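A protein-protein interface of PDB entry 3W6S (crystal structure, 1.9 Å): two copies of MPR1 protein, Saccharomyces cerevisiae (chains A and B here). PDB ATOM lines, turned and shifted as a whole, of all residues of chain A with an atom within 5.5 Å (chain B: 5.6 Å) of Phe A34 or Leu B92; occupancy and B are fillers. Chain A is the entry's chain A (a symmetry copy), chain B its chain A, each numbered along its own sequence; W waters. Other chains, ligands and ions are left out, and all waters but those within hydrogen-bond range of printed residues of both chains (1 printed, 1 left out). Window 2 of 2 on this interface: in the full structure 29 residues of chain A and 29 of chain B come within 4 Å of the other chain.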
ATOM      1  N   PRO A  32      13.026 -33.102 -20.405  1.00  0.00           N
ATOM      2  CA  PRO A  32      12.073 -32.030 -20.075  1.00  0.00           C
ATOM      3  C   PRO A  32      11.949 -30.952 -21.143  1.00  0.00           C
ATOM      4  O   PRO A  32      12.929 -30.511 -21.719  1.00  0.00           O
ATOM      5  CB  PRO A  32      12.655 -31.402 -18.810  1.00  0.00           C
ATOM      6  CG  PRO A  32      13.601 -32.412 -18.251  1.00  0.00           C
ATOM      7  CD  PRO A  32      14.081 -33.251 -19.392  1.00  0.00           C
ATOM      8  N   THR A  33      10.724 -30.522 -21.384  1.00  0.00           N
ATOM      9  CA  THR A  33      10.436 -29.522 -22.393  1.00  0.00           C
ATOM     10  C   THR A  33      10.631 -28.111 -21.858  1.00  0.00           C
ATOM     11  O   THR A  33      11.118 -27.231 -22.566  1.00  0.00           O
ATOM     12  CB  THR A  33       8.986 -29.675 -22.840  1.00  0.00           C
ATOM     13  OG1 THR A  33       8.835 -30.939 -23.496  1.00  0.00           O
ATOM     14  CG2 THR A  33       8.560 -28.545 -23.773  1.00  0.00           C
ATOM     15  N   PHE A  34      10.254 -27.897 -20.604  1.00  0.00           N
ATOM     16  CA  PHE A  34      10.167 -26.548 -20.058  1.00  0.00           C
ATOM     17  C   PHE A  34      11.369 -26.122 -19.208  1.00  0.00           C
ATOM     18  O   PHE A  34      11.515 -24.946 -18.892  1.00  0.00           O
ATOM     19  CB  PHE A  34       8.884 -26.427 -19.233  1.00  0.00           C
ATOM     20  CG  PHE A  34       7.619 -26.469 -20.059  1.00  0.00           C
ATOM     21  CD1 PHE A  34       7.032 -27.673 -20.410  1.00  0.00           C
ATOM     22  CD2 PHE A  34       7.014 -25.304 -20.479  1.00  0.00           C
ATOM     23  CE1 PHE A  34       5.876 -27.705 -21.170  1.00  0.00           C
ATOM     24  CE2 PHE A  34       5.852 -25.339 -21.235  1.00  0.00           C
ATOM     25  CZ  PHE A  34       5.288 -26.538 -21.577  1.00  0.00           C
ATOM     26  N   PHE A  35      12.232 -27.060 -18.843  1.00  0.00           N
ATOM     27  CA  PHE A  35      13.319 -26.757 -17.925  1.00  0.00           C
ATOM     28  C   PHE A  35      14.648 -27.252 -18.450  1.00  0.00           C
ATOM     29  O   PHE A  35      14.744 -28.352 -18.983  1.00  0.00           O
ATOM     30  CB  PHE A  35      13.053 -27.407 -16.575  1.00  0.00           C
ATOM     31  CG  PHE A  35      11.798 -26.928 -15.915  1.00  0.00           C
ATOM     32  CD1 PHE A  35      11.799 -25.786 -15.150  1.00  0.00           C
ATOM     33  CD2 PHE A  35      10.615 -27.614 -16.072  1.00  0.00           C
ATOM     34  CE1 PHE A  35      10.654 -25.348 -14.546  1.00  0.00           C
ATOM     35  CE2 PHE A  35       9.468 -27.175 -15.474  1.00  0.00           C
ATOM     36  CZ  PHE A  35       9.485 -26.044 -14.708  1.00  0.00           C
ATOM     37  N   GLN A  36      15.676 -26.433 -18.294  1.00  0.00           N
ATOM     38  CA  GLN A  36      16.997 -26.803 -18.741  1.00  0.00           C
ATOM     39  C   GLN A  36      17.730 -27.571 -17.651  1.00  0.00           C
ATOM     40  O   GLN A  36      17.313 -27.581 -16.494  1.00  0.00           O
ATOM     41  CB  GLN A  36      17.795 -25.549 -19.097  1.00  0.00           C
ATOM     42  CG  GLN A  36      17.466 -24.957 -20.454  1.00  0.00           C
ATOM     43  N   PRO A 142       4.903 -33.254 -22.479  1.00  0.00           N
ATOM     44  CA  PRO A 142       5.615 -31.986 -22.242  1.00  0.00           C
ATOM     45  C   PRO A 142       5.151 -31.094 -21.098  1.00  0.00           C
ATOM     46  O   PRO A 142       6.014 -30.602 -20.366  1.00  0.00           O
ATOM     47  CB  PRO A 142       5.434 -31.261 -23.568  1.00  0.00           C
ATOM     48  CG  PRO A 142       5.556 -32.361 -24.546  1.00  0.00           C
ATOM     49  CD  PRO A 142       4.777 -33.501 -23.926  1.00  0.00           C
ATOM     50  N   ARG A 143       3.854 -30.835 -20.960  1.00  0.00           N
ATOM     51  CA  ARG A 143       3.414 -29.927 -19.908  1.00  0.00           C
ATOM     52  C   ARG A 143       3.722 -30.477 -18.529  1.00  0.00           C
ATOM     53  O   ARG A 143       3.827 -29.727 -17.568  1.00  0.00           O
ATOM     54  CB  ARG A 143       1.933 -29.631 -20.035  1.00  0.00           C
ATOM     55  CG  ARG A 143       1.627 -28.767 -21.223  1.00  0.00           C
ATOM     56  CD  ARG A 143       0.222 -28.235 -21.164  1.00  0.00           C
ATOM     57  NE  ARG A 143      -0.037 -27.327 -22.274  1.00  0.00           N
ATOM     58  CZ  ARG A 143       0.234 -26.028 -22.258  1.00  0.00           C
ATOM     59  NH1 ARG A 143       0.773 -25.467 -21.186  1.00  0.00           N
ATOM     60  NH2 ARG A 143      -0.038 -25.285 -23.313  1.00  0.00           N
ATOM     61  N   CYS A 144       3.902 -31.787 -18.440  1.00  0.00           N
ATOM     62  CA  CYS A 144       4.183 -32.417 -17.161  1.00  0.00           C
ATOM     63  C   CYS A 144       5.529 -33.116 -17.165  1.00  0.00           C
ATOM     64  O   CYS A 144       5.794 -33.933 -16.304  1.00  0.00           O
ATOM     65  CB  CYS A 144       3.086 -33.432 -16.813  1.00  0.00           C
ATOM     66  SG  CYS A 144       1.412 -32.724 -16.797  1.00  0.00           S
ATOM     67  N   SER A 145       6.376 -32.787 -18.133  1.00  0.00           N
ATOM     68  CA  SER A 145       7.599 -33.542 -18.386  1.00  0.00           C
ATOM     69  C   SER A 145       8.705 -33.249 -17.385  1.00  0.00           C
ATOM     70  O   SER A 145       9.784 -33.828 -17.469  1.00  0.00           O
ATOM     71  CB  SER A 145       8.107 -33.252 -19.796  1.00  0.00           C
ATOM     72  OG  SER A 145       8.351 -31.876 -19.960  1.00  0.00           O
ATOM     73  N   ILE B  83      -6.237 -29.583 -26.795  1.00  0.00           N
ATOM     74  CA  ILE B  83      -4.813 -29.543 -26.498  1.00  0.00           C
ATOM     75  C   ILE B  83      -4.325 -28.105 -26.531  1.00  0.00           C
ATOM     76  O   ILE B  83      -3.591 -27.667 -25.643  1.00  0.00           O
ATOM     77  CB  ILE B  83      -4.017 -30.365 -27.514  1.00  0.00           C
ATOM     78  CG1 ILE B  83      -4.188 -31.852 -27.220  1.00  0.00           C
ATOM     79  CG2 ILE B  83      -2.535 -29.994 -27.468  1.00  0.00           C
ATOM     80  CD1 ILE B  83      -3.609 -32.736 -28.289  1.00  0.00           C
ATOM     81  N   GLU B  84      -4.740 -27.377 -27.565  1.00  0.00           N
ATOM     82  CA  GLU B  84      -4.334 -25.992 -27.746  1.00  0.00           C
ATOM     83  C   GLU B  84      -4.787 -25.097 -26.603  1.00  0.00           C
ATOM     84  O   GLU B  84      -4.151 -24.091 -26.324  1.00  0.00           O
ATOM     85  CB  GLU B  84      -4.852 -25.469 -29.082  1.00  0.00           C
ATOM     86  CG  GLU B  84      -4.218 -26.159 -30.277  1.00  0.00           C
ATOM     87  N   PRO B  90      -1.755 -33.190 -21.010  1.00  0.00           N
ATOM     88  CA  PRO B  90      -0.322 -32.895 -20.868  1.00  0.00           C
ATOM     89  C   PRO B  90       0.384 -32.543 -22.175  1.00  0.00           C
ATOM     90  O   PRO B  90       1.487 -32.004 -22.138  1.00  0.00           O
ATOM     91  CB  PRO B  90       0.247 -34.200 -20.307  1.00  0.00           C
ATOM     92  CG  PRO B  90      -0.685 -35.256 -20.801  1.00  0.00           C
ATOM     93  CD  PRO B  90      -2.045 -34.615 -20.783  1.00  0.00           C
ATOM     94  N   GLN B  91      -0.239 -32.827 -23.313  1.00  0.00           N
ATOM     95  CA  GLN B  91       0.355 -32.502 -24.604  1.00  0.00           C
ATOM     96  C   GLN B  91       0.532 -31.015 -24.735  1.00  0.00           C
ATOM     97  O   GLN B  91      -0.307 -30.245 -24.292  1.00  0.00           O
ATOM     98  CB  GLN B  91      -0.531 -32.990 -25.748  1.00  0.00           C
ATOM     99  CG  GLN B  91      -0.454 -34.493 -26.000  1.00  0.00           C
ATOM    100  CD  GLN B  91      -1.264 -35.287 -24.998  1.00  0.00           C
ATOM    101  OE1 GLN B  91      -2.282 -34.811 -24.506  1.00  0.00           O
ATOM    102  NE2 GLN B  91      -0.813 -36.491 -24.677  1.00  0.00           N
ATOM    103  N   LEU B  92       1.615 -30.614 -25.377  1.00  0.00           N
ATOM    104  CA  LEU B  92       1.850 -29.215 -25.661  1.00  0.00           C
ATOM    105  C   LEU B  92       1.377 -28.914 -27.079  1.00  0.00           C
ATOM    106  O   LEU B  92       0.740 -27.898 -27.343  1.00  0.00           O
ATOM    107  CB  LEU B  92       3.338 -28.927 -25.540  1.00  0.00           C
ATOM    108  CG  LEU B  92       3.714 -27.464 -25.737  1.00  0.00           C
ATOM    109  CD1 LEU B  92       2.914 -26.585 -24.781  1.00  0.00           C
ATOM    110  CD2 LEU B  92       5.200 -27.298 -25.512  1.00  0.00           C
ATOM    111  N   HIS B  93       1.675 -29.838 -27.982  1.00  0.00           N
ATOM    112  CA  HIS B  93       1.456 -29.641 -29.406  1.00  0.00           C
ATOM    113  C   HIS B  93       0.287 -30.439 -29.966  1.00  0.00           C
ATOM    114  O   HIS B  93      -0.093 -31.467 -29.424  1.00  0.00           O
ATOM    115  CB  HIS B  93       2.730 -30.021 -30.146  1.00  0.00           C
ATOM    116  CG  HIS B  93       3.875 -29.125 -29.832  1.00  0.00           C
ATOM    117  ND1 HIS B  93       5.041 -29.572 -29.244  1.00  0.00           N
ATOM    118  CD2 HIS B  93       4.024 -27.789 -29.991  1.00  0.00           C
ATOM    119  CE1 HIS B  93       5.862 -28.553 -29.072  1.00  0.00           C
ATOM    120  NE2 HIS B  93       5.266 -27.460 -29.516  1.00  0.00           N
ATOM    121  N   SER B  94      -0.271 -29.958 -31.070  1.00  0.00           N
ATOM    122  CA  SER B  94      -1.328 -30.670 -31.767  1.00  0.00           C
ATOM    123  C   SER B  94      -0.752 -31.893 -32.446  1.00  0.00           C
ATOM    124  O   SER B  94       0.387 -31.882 -32.906  1.00  0.00           O
ATOM    125  CB  SER B  94      -1.970 -29.777 -32.819  1.00  0.00           C
ATOM    126  OG  SER B  94      -2.754 -28.770 -32.210  1.00  0.00           O
ATOM    127  N   ILE B 215       2.283 -27.787 -16.011  1.00  0.00           N
ATOM    128  CA  ILE B 215       2.352 -26.396 -16.409  1.00  0.00           C
ATOM    129  C   ILE B 215       1.211 -26.144 -17.378  1.00  0.00           C
ATOM    130  O   ILE B 215       1.205 -26.683 -18.483  1.00  0.00           O
ATOM    131  CB  ILE B 215       3.666 -26.083 -17.126  1.00  0.00           C
ATOM    132  CG1 ILE B 215       4.848 -26.567 -16.285  1.00  0.00           C
ATOM    133  CG2 ILE B 215       3.775 -24.578 -17.418  1.00  0.00           C
ATOM    134  CD1 ILE B 215       4.780 -26.112 -14.822  1.00  0.00           C
HETATM  135  O   HOH W   1      -2.752 -29.043 -23.486  1.00  0.00           O
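Printed residues of chain B within 4 Å of Phe A34: Leu B92 (3.99 Å).
Of the printed residues of chain B, Arg A143 touches Pro B90 (2.9 Å), Gln B91 (3.6 Å), Leu B92 (3.5 Å) and Ile B215 (2.9 Å).
Printed residues of chain B within 4 Å of Cys A144: Pro B90 (3.98 Å).
Ser A145 touches none of the printed residues of chain B.
Printed residues of chain A within 4 Å of Leu B92: Thr A33, Phe A34, Pro A142 and Arg A143.
Ser B94 touches none of the printed residues of chain A.
Printed residues of chain A within 4 Å of Ile B215: Arg A143.
O of Arg A143 sits at hydrogen-bond distance from N of Ile B215.
N of Arg A143 is in hydrogen-bond range of O of Pro B90.
N of Thr A33 sits at hydrogen-bond distance from OG of Ser A145, at 3.1 Å.
O of Pro A142 is in hydrogen-bond range of OG of Ser A145, at 2.7 Å.
No position is printed for both chains.
Of the 9 pairs that touch across the chains among the printed residues, none has its exchanged pair printed and touching as well.
Among the printed residues, pairs that only touch across the chains: Arg A143 with Leu B92 (3.5 Å), Arg A143 with Gln B91 (3.6 Å), Pro A142 with Pro B90 (3.7 Å), Pro A142 with Leu B92 (3.7 Å), Cys A144 with Pro B90 (3.98 Å), Thr A33 with Leu B92 (3.98 Å) and Phe A34 with Leu B92 (3.99 Å).
Hydrophobic or aromatic side chains of chain B within 4 Å of the printed part of chain A: Pro B90, Leu B92 and Ile B215.
Hydrophobic or aromatic side chains of chain A within 4 Å of the printed part of chain B: Phe A34 and Pro A142.
Among the printed residues, 9 pairs touch across the chains.
Among the printed residues, no Asp or Glu carboxylate lies within 4 Å of a Lys or Arg side-chain nitrogen of the other chain.
Water W1 lies within hydrogen-bond range of the backbone carbonyl oxygen of Ile B83 (2.7 Å), the backbone carbonyl oxygen of Gln B91 (2.8 Å) and the guanidinium group of Arg A143 (3.4 Å).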
